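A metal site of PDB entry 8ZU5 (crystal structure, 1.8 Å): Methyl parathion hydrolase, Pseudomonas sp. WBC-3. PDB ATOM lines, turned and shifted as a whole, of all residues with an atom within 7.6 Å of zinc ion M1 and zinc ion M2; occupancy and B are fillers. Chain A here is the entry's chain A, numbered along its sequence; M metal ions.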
ATOM      1  N   LEU A  32     -17.963  10.624 -17.344  1.00  0.00           N
ATOM      2  CA  LEU A  32     -18.732  11.870 -17.367  1.00  0.00           C
ATOM      3  C   LEU A  32     -19.119  12.257 -18.790  1.00  0.00           C
ATOM      4  O   LEU A  32     -18.280  12.170 -19.704  1.00  0.00           O
ATOM      5  CB  LEU A  32     -17.967  13.035 -16.711  1.00  0.00           C
ATOM      6  CG  LEU A  32     -17.564  12.868 -15.240  1.00  0.00           C
ATOM      7  CD1 LEU A  32     -16.785  14.065 -14.678  1.00  0.00           C
ATOM      8  CD2 LEU A  32     -18.811  12.589 -14.400  1.00  0.00           C
ATOM      9  N   THR A  60     -13.110   9.974 -15.986  1.00  0.00           N
ATOM     10  CA  THR A  60     -12.508  11.161 -15.361  1.00  0.00           C
ATOM     11  C   THR A  60     -11.983  10.782 -13.975  1.00  0.00           C
ATOM     12  O   THR A  60     -12.747  10.278 -13.139  1.00  0.00           O
ATOM     13  CB  THR A  60     -13.517  12.298 -15.265  1.00  0.00           C
ATOM     14  OG1 THR A  60     -14.091  12.576 -16.552  1.00  0.00           O
ATOM     15  CG2 THR A  60     -12.860  13.564 -14.675  1.00  0.00           C
ATOM     16  N   SER A  61     -10.689  11.001 -13.724  1.00  0.00           N
ATOM     17  CA  SER A  61     -10.297  10.649 -12.366  1.00  0.00           C
ATOM     18  C   SER A  61     -10.692  11.732 -11.350  1.00  0.00           C
ATOM     19  O   SER A  61     -11.057  12.849 -11.703  1.00  0.00           O
ATOM     20  CB  SER A  61      -8.814  10.222 -12.291  1.00  0.00           C
ATOM     21  OG  SER A  61      -7.925  10.833 -13.191  1.00  0.00           O
ATOM     22  N   VAL A  62     -10.709  11.325 -10.080  1.00  0.00           N
ATOM     23  CA  VAL A  62     -11.093  12.168  -8.936  1.00  0.00           C
ATOM     24  C   VAL A  62      -9.984  11.990  -7.922  1.00  0.00           C
ATOM     25  O   VAL A  62      -9.778  10.868  -7.444  1.00  0.00           O
ATOM     26  CB  VAL A  62     -12.441  11.732  -8.318  1.00  0.00           C
ATOM     27  CG1 VAL A  62     -12.778  12.572  -7.023  1.00  0.00           C
ATOM     28  CG2 VAL A  62     -13.582  11.749  -9.391  1.00  0.00           C
ATOM     29  N   ASP A  77      -8.984  18.149  -0.264  1.00  0.00           N
ATOM     30  CA  ASP A  77     -10.112  17.439  -0.859  1.00  0.00           C
ATOM     31  C   ASP A  77     -10.080  15.949  -0.531  1.00  0.00           C
ATOM     32  O   ASP A  77      -9.011  15.395  -0.252  1.00  0.00           O
ATOM     33  CB  ASP A  77     -10.158  17.671  -2.356  1.00  0.00           C
ATOM     34  CG  ASP A  77     -10.472  19.110  -2.717  1.00  0.00           C
ATOM     35  OD1 ASP A  77     -10.825  19.932  -1.818  1.00  0.00           O
ATOM     36  OD2 ASP A  77     -10.315  19.419  -3.917  1.00  0.00           O
ATOM     37  N   THR A 111     -11.038  22.591  -1.639  1.00  0.00           N
ATOM     38  CA  THR A 111     -11.080  23.538  -2.741  1.00  0.00           C
ATOM     39  C   THR A 111     -12.495  24.056  -2.923  1.00  0.00           C
ATOM     40  O   THR A 111     -12.704  25.260  -3.138  1.00  0.00           O
ATOM     41  CB  THR A 111     -10.528  22.940  -4.040  1.00  0.00           C
ATOM     42  OG1 THR A 111     -11.308  21.831  -4.431  1.00  0.00           O
ATOM     43  CG2 THR A 111      -9.028  22.521  -3.832  1.00  0.00           C
ATOM     44  N   HIS A 112     -13.490  23.196  -2.743  1.00  0.00           N
ATOM     45  CA  HIS A 112     -14.901  23.552  -2.833  1.00  0.00           C
ATOM     46  C   HIS A 112     -15.710  22.373  -2.338  1.00  0.00           C
ATOM     47  O   HIS A 112     -15.152  21.314  -2.028  1.00  0.00           O
ATOM     48  CB  HIS A 112     -15.296  23.946  -4.248  1.00  0.00           C
ATOM     49  CG  HIS A 112     -15.227  22.824  -5.256  1.00  0.00           C
ATOM     50  ND1 HIS A 112     -14.072  22.147  -5.534  1.00  0.00           N
ATOM     51  CD2 HIS A 112     -16.151  22.375  -6.145  1.00  0.00           C
ATOM     52  CE1 HIS A 112     -14.289  21.301  -6.532  1.00  0.00           C
ATOM     53  NE2 HIS A 112     -15.554  21.418  -6.915  1.00  0.00           N
ATOM     54  N   MET A 113     -17.040  22.523  -2.337  1.00  0.00           N
ATOM     55  CA  MET A 113     -17.885  21.600  -1.590  1.00  0.00           C
ATOM     56  C   MET A 113     -18.724  20.674  -2.474  1.00  0.00           C
ATOM     57  O   MET A 113     -19.725  20.117  -1.995  1.00  0.00           O
ATOM     58  CB  MET A 113     -18.761  22.423  -0.668  1.00  0.00           C
ATOM     59  CG  MET A 113     -17.927  22.884   0.488  1.00  0.00           C
ATOM     60  SD  MET A 113     -18.791  23.690   1.801  1.00  0.00           S
ATOM     61  CE  MET A 113     -17.400  24.259   2.786  1.00  0.00           C
ATOM     62  N   HIS A 114     -18.378  20.529  -3.758  1.00  0.00           N
ATOM     63  CA  HIS A 114     -19.076  19.540  -4.593  1.00  0.00           C
ATOM     64  C   HIS A 114     -18.866  18.136  -4.015  1.00  0.00           C
ATOM     65  O   HIS A 114     -17.903  17.911  -3.270  1.00  0.00           O
ATOM     66  CB  HIS A 114     -18.555  19.604  -6.026  1.00  0.00           C
ATOM     67  CG  HIS A 114     -19.207  20.650  -6.895  1.00  0.00           C
ATOM     68  ND1 HIS A 114     -18.704  21.010  -8.121  1.00  0.00           N
ATOM     69  CD2 HIS A 114     -20.301  21.427  -6.688  1.00  0.00           C
ATOM     70  CE1 HIS A 114     -19.447  21.970  -8.637  1.00  0.00           C
ATOM     71  NE2 HIS A 114     -20.440  22.227  -7.806  1.00  0.00           N
ATOM     72  N   PRO A 115     -19.753  17.180  -4.323  1.00  0.00           N
ATOM     73  CA  PRO A 115     -19.755  15.905  -3.586  1.00  0.00           C
ATOM     74  C   PRO A 115     -18.496  15.078  -3.719  1.00  0.00           C
ATOM     75  O   PRO A 115     -18.138  14.353  -2.783  1.00  0.00           O
ATOM     76  CB  PRO A 115     -20.958  15.153  -4.180  1.00  0.00           C
ATOM     77  CG  PRO A 115     -21.800  16.157  -4.806  1.00  0.00           C
ATOM     78  CD  PRO A 115     -20.859  17.238  -5.301  1.00  0.00           C
ATOM     79  N   ASP A 116     -17.831  15.146  -4.870  1.00  0.00           N
ATOM     80  CA  ASP A 116     -16.615  14.405  -5.184  1.00  0.00           C
ATOM     81  C   ASP A 116     -15.363  15.003  -4.559  1.00  0.00           C
ATOM     82  O   ASP A 116     -14.237  14.549  -4.843  1.00  0.00           O
ATOM     83  CB  ASP A 116     -16.467  14.291  -6.716  1.00  0.00           C
ATOM     84  CG  ASP A 116     -16.629  15.625  -7.435  1.00  0.00           C
ATOM     85  OD1 ASP A 116     -17.700  16.264  -7.265  1.00  0.00           O
ATOM     86  OD2 ASP A 116     -15.690  16.049  -8.169  1.00  0.00           O
ATOM     87  N   HIS A 117     -15.552  16.007  -3.709  1.00  0.00           N
ATOM     88  CA  HIS A 117     -14.501  16.641  -2.934  1.00  0.00           C
ATOM     89  C   HIS A 117     -14.787  16.634  -1.435  1.00  0.00           C
ATOM     90  O   HIS A 117     -13.838  16.631  -0.639  1.00  0.00           O
ATOM     91  CB  HIS A 117     -14.330  18.096  -3.399  1.00  0.00           C
ATOM     92  CG  HIS A 117     -13.905  18.205  -4.828  1.00  0.00           C
ATOM     93  ND1 HIS A 117     -12.604  18.485  -5.191  1.00  0.00           N
ATOM     94  CD2 HIS A 117     -14.607  18.057  -5.986  1.00  0.00           C
ATOM     95  CE1 HIS A 117     -12.527  18.530  -6.509  1.00  0.00           C
ATOM     96  NE2 HIS A 117     -13.725  18.241  -7.013  1.00  0.00           N
ATOM     97  N   TRP A 144     -23.178  26.617   0.347  1.00  0.00           N
ATOM     98  CA  TRP A 144     -23.607  25.222   0.273  1.00  0.00           C
ATOM     99  C   TRP A 144     -24.310  24.740   1.536  1.00  0.00           C
ATOM    100  O   TRP A 144     -25.081  23.776   1.456  1.00  0.00           O
ATOM    101  CB  TRP A 144     -22.418  24.307  -0.045  1.00  0.00           C
ATOM    102  CG  TRP A 144     -21.877  24.525  -1.438  1.00  0.00           C
ATOM    103  CD1 TRP A 144     -20.675  25.086  -1.761  1.00  0.00           C
ATOM    104  CD2 TRP A 144     -22.509  24.171  -2.688  1.00  0.00           C
ATOM    105  NE1 TRP A 144     -20.535  25.131  -3.151  1.00  0.00           N
ATOM    106  CE2 TRP A 144     -21.637  24.569  -3.728  1.00  0.00           C
ATOM    107  CE3 TRP A 144     -23.719  23.566  -3.025  1.00  0.00           C
ATOM    108  CZ2 TRP A 144     -21.941  24.373  -5.081  1.00  0.00           C
ATOM    109  CZ3 TRP A 144     -24.023  23.363  -4.371  1.00  0.00           C
ATOM    110  CH2 TRP A 144     -23.137  23.774  -5.384  1.00  0.00           C
ATOM    111  N   PHE A 161     -26.380  18.206  -4.356  1.00  0.00           N
ATOM    112  CA  PHE A 161     -25.140  18.879  -3.994  1.00  0.00           C
ATOM    113  C   PHE A 161     -25.246  19.492  -2.603  1.00  0.00           C
ATOM    114  O   PHE A 161     -24.325  19.351  -1.761  1.00  0.00           O
ATOM    115  CB  PHE A 161     -24.794  19.968  -5.005  1.00  0.00           C
ATOM    116  CG  PHE A 161     -24.381  19.440  -6.345  1.00  0.00           C
ATOM    117  CD1 PHE A 161     -23.852  18.179  -6.472  1.00  0.00           C
ATOM    118  CD2 PHE A 161     -24.525  20.219  -7.484  1.00  0.00           C
ATOM    119  CE1 PHE A 161     -23.465  17.690  -7.717  1.00  0.00           C
ATOM    120  CE2 PHE A 161     -24.146  19.738  -8.721  1.00  0.00           C
ATOM    121  CZ  PHE A 161     -23.617  18.470  -8.841  1.00  0.00           C
ATOM    122  N   HIS A 199     -16.001  28.662 -10.105  1.00  0.00           N
ATOM    123  CA  HIS A 199     -16.573  27.301 -10.313  1.00  0.00           C
ATOM    124  C   HIS A 199     -17.625  27.170  -9.218  1.00  0.00           C
ATOM    125  O   HIS A 199     -18.710  26.632  -9.491  1.00  0.00           O
ATOM    126  CB  HIS A 199     -15.484  26.246 -10.134  1.00  0.00           C
ATOM    127  CG  HIS A 199     -15.976  24.837 -10.124  1.00  0.00           C
ATOM    128  ND1 HIS A 199     -16.648  24.269 -11.191  1.00  0.00           N
ATOM    129  CD2 HIS A 199     -15.872  23.889  -9.193  1.00  0.00           C
ATOM    130  CE1 HIS A 199     -16.940  23.016 -10.890  1.00  0.00           C
ATOM    131  NE2 HIS A 199     -16.485  22.761  -9.689  1.00  0.00           N
ATOM    132  N   THR A 200     -17.282  27.595  -7.991  1.00  0.00           N
ATOM    133  CA  THR A 200     -18.240  27.689  -6.886  1.00  0.00           C
ATOM    134  C   THR A 200     -18.016  29.055  -6.276  1.00  0.00           C
ATOM    135  O   THR A 200     -16.951  29.638  -6.492  1.00  0.00           O
ATOM    136  CB  THR A 200     -18.020  26.575  -5.854  1.00  0.00           C
ATOM    137  OG1 THR A 200     -16.689  26.708  -5.380  1.00  0.00           O
ATOM    138  CG2 THR A 200     -18.264  25.190  -6.441  1.00  0.00           C
ATOM    139  N   HIS A 203     -14.673  28.751  -4.357  1.00  0.00           N
ATOM    140  CA  HIS A 203     -13.630  27.834  -4.800  1.00  0.00           C
ATOM    141  C   HIS A 203     -12.255  28.422  -4.510  1.00  0.00           C
ATOM    142  O   HIS A 203     -11.976  29.584  -4.844  1.00  0.00           O
ATOM    143  CB  HIS A 203     -13.737  27.553  -6.295  1.00  0.00           C
ATOM    144  CG  HIS A 203     -12.727  26.553  -6.777  1.00  0.00           C
ATOM    145  ND1 HIS A 203     -11.421  26.891  -7.055  1.00  0.00           N
ATOM    146  CD2 HIS A 203     -12.877  25.262  -7.161  1.00  0.00           C
ATOM    147  CE1 HIS A 203     -10.776  25.821  -7.487  1.00  0.00           C
ATOM    148  NE2 HIS A 203     -11.633  24.822  -7.572  1.00  0.00           N
ATOM    149  N   GLY A 219      -7.743  22.505  -7.643  1.00  0.00           N
ATOM    150  CA  GLY A 219      -9.111  22.065  -7.465  1.00  0.00           C
ATOM    151  C   GLY A 219      -9.756  21.802  -8.821  1.00  0.00           C
ATOM    152  O   GLY A 219      -9.238  21.015  -9.632  1.00  0.00           O
ATOM    153  N   ASP A 220     -10.893  22.456  -9.071  1.00  0.00           N
ATOM    154  CA  ASP A 220     -11.665  22.293 -10.299  1.00  0.00           C
ATOM    155  C   ASP A 220     -11.568  23.506 -11.211  1.00  0.00           C
ATOM    156  O   ASP A 220     -12.557  23.884 -11.876  1.00  0.00           O
ATOM    157  CB  ASP A 220     -13.122  21.984  -9.947  1.00  0.00           C
ATOM    158  CG  ASP A 220     -13.313  20.537  -9.572  1.00  0.00           C
ATOM    159  OD1 ASP A 220     -12.300  19.852  -9.408  1.00  0.00           O
ATOM    160  OD2 ASP A 220     -14.469  20.105  -9.404  1.00  0.00           O
ATOM    161  N   LEU A 221     -10.421  24.184 -11.223  1.00  0.00           N
ATOM    162  CA  LEU A 221     -10.263  25.263 -12.198  1.00  0.00           C
ATOM    163  C   LEU A 221     -10.183  24.737 -13.615  1.00  0.00           C
ATOM    164  O   LEU A 221     -10.332  25.527 -14.547  1.00  0.00           O
ATOM    165  CB  LEU A 221      -9.036  26.114 -11.928  1.00  0.00           C
ATOM    166  CG  LEU A 221      -9.122  27.154 -10.818  1.00  0.00           C
ATOM    167  CD1 LEU A 221      -7.793  27.894 -10.716  1.00  0.00           C
ATOM    168  CD2 LEU A 221     -10.239  28.095 -11.235  1.00  0.00           C
ATOM    169  N   ILE A 222      -9.905  23.450 -13.791  1.00  0.00           N
ATOM    170  CA  ILE A 222     -10.016  22.782 -15.079  1.00  0.00           C
ATOM    171  C   ILE A 222     -10.710  21.445 -14.867  1.00  0.00           C
ATOM    172  O   ILE A 222     -10.447  20.730 -13.891  1.00  0.00           O
ATOM    173  CB  ILE A 222      -8.645  22.589 -15.754  1.00  0.00           C
ATOM    174  CG1 ILE A 222      -8.849  22.028 -17.159  1.00  0.00           C
ATOM    175  CG2 ILE A 222      -7.750  21.690 -14.927  1.00  0.00           C
ATOM    176  CD1 ILE A 222      -7.626  22.089 -18.017  1.00  0.00           C
ATOM    177  N   LEU A 223     -11.631  21.124 -15.758  1.00  0.00           N
ATOM    178  CA  LEU A 223     -12.436  19.917 -15.655  1.00  0.00           C
ATOM    179  C   LEU A 223     -12.198  18.940 -16.803  1.00  0.00           C
ATOM    180  O   LEU A 223     -12.251  17.726 -16.580  1.00  0.00           O
ATOM    181  CB  LEU A 223     -13.919  20.303 -15.602  1.00  0.00           C
ATOM    182  CG  LEU A 223     -14.281  21.166 -14.368  1.00  0.00           C
ATOM    183  CD1 LEU A 223     -15.689  21.798 -14.494  1.00  0.00           C
ATOM    184  CD2 LEU A 223     -14.147  20.369 -13.035  1.00  0.00           C
ATOM    185  N   LEU A 238     -21.719  23.373 -14.824  1.00  0.00           N
ATOM    186  CA  LEU A 238     -21.433  23.202 -13.397  1.00  0.00           C
ATOM    187  C   LEU A 238     -20.758  24.410 -12.781  1.00  0.00           C
ATOM    188  O   LEU A 238     -20.633  24.451 -11.535  1.00  0.00           O
ATOM    189  CB  LEU A 238     -20.511  22.022 -13.157  1.00  0.00           C
ATOM    190  CG  LEU A 238     -20.859  20.607 -13.575  1.00  0.00           C
ATOM    191  CD1 LEU A 238     -19.586  19.784 -13.311  1.00  0.00           C
ATOM    192  CD2 LEU A 238     -22.072  20.118 -12.787  1.00  0.00           C
ATOM    193  N   ASP A 239     -20.280  25.361 -13.578  1.00  0.00           N
ATOM    194  CA  ASP A 239     -19.598  26.525 -13.034  1.00  0.00           C
ATOM    195  C   ASP A 239     -20.607  27.567 -12.581  1.00  0.00           C
ATOM    196  O   ASP A 239     -21.485  27.961 -13.357  1.00  0.00           O
ATOM    197  CB  ASP A 239     -18.613  27.111 -14.044  1.00  0.00           C
ATOM    198  CG  ASP A 239     -17.540  26.142 -14.441  1.00  0.00           C
ATOM    199  OD1 ASP A 239     -16.759  25.752 -13.546  1.00  0.00           O
ATOM    200  OD2 ASP A 239     -17.437  25.809 -15.654  1.00  0.00           O
ATOM    201  N   SER A 266      -7.913  18.223  -9.609  1.00  0.00           N
ATOM    202  CA  SER A 266      -8.661  17.059  -9.129  1.00  0.00           C
ATOM    203  C   SER A 266      -9.015  16.090 -10.246  1.00  0.00           C
ATOM    204  O   SER A 266      -9.042  14.866 -10.046  1.00  0.00           O
ATOM    205  CB  SER A 266      -9.955  17.514  -8.450  1.00  0.00           C
ATOM    206  OG  SER A 266      -9.734  18.558  -7.496  1.00  0.00           O
ATOM    207  N   HIS A 267      -9.339  16.623 -11.427  1.00  0.00           N
ATOM    208  CA  HIS A 267      -9.819  15.794 -12.530  1.00  0.00           C
ATOM    209  C   HIS A 267      -8.888  15.736 -13.725  1.00  0.00           C
ATOM    210  O   HIS A 267      -9.300  15.235 -14.786  1.00  0.00           O
ATOM    211  CB  HIS A 267     -11.215  16.271 -12.949  1.00  0.00           C
ATOM    212  CG  HIS A 267     -12.150  16.329 -11.797  1.00  0.00           C
ATOM    213  ND1 HIS A 267     -12.457  15.211 -11.039  1.00  0.00           N
ATOM    214  CD2 HIS A 267     -12.791  17.365 -11.215  1.00  0.00           C
ATOM    215  CE1 HIS A 267     -13.285  15.554 -10.071  1.00  0.00           C
ATOM    216  NE2 HIS A 267     -13.478  16.858 -10.146  1.00  0.00           N
HETATM  217 ZN    ZN M   1     -14.997  17.954  -8.888  1.00  0.00          ZN
HETATM  218 ZN    ZN M   2     -16.568  20.706  -8.904  1.00  0.00          ZN
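N of Asp 220 lies within hydrogen-bond range of NE2 of His 203 (2.9 Å).
OD2 of Asp 77 is in hydrogen-bond range of ND1 of His 117 (2.8 Å).
OG1 of Thr 111 lies within hydrogen-bond range of ND1 of His 112 (3.0 Å).
The side-chain carboxylate of Asp 220 sits close to the side-chain hydroxyl of Ser 266 (3.5 Å).
ND1 of His 267 is in hydrogen-bond range of O of Ser 61 (2.8 Å).
A ring nitrogen (ND1) of His 199 sits at hydrogen-bond distance from the side-chain carboxylate (OD1) of Asp 239.
Along chain A the residues within 4 Å of zinc ion M1 span positions 116 to 267.
Along chain A the residues within 4 Å of zinc ion M2 span positions 112 to 220.
Zinc ion M1 is bound by OD2 of Asp 116 (2.2 Å), NE2 of His 267 (2.3 Å), OD2 of Asp 220 (2.3 Å) and NE2 of His 117 (2.3 Å).
Zinc ion M2 is bound by NE2 of His 199.
OD2 of Asp 220 is bound to zinc ion M2 (2.2 Å).
Zinc ion M2 is bound by a ring nitrogen (ND1) of His 114 (2.3 Å).
Zinc ion M2 is bound by NE2 of His 112.
Zinc ion M2 has four donor atoms within binding distance.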
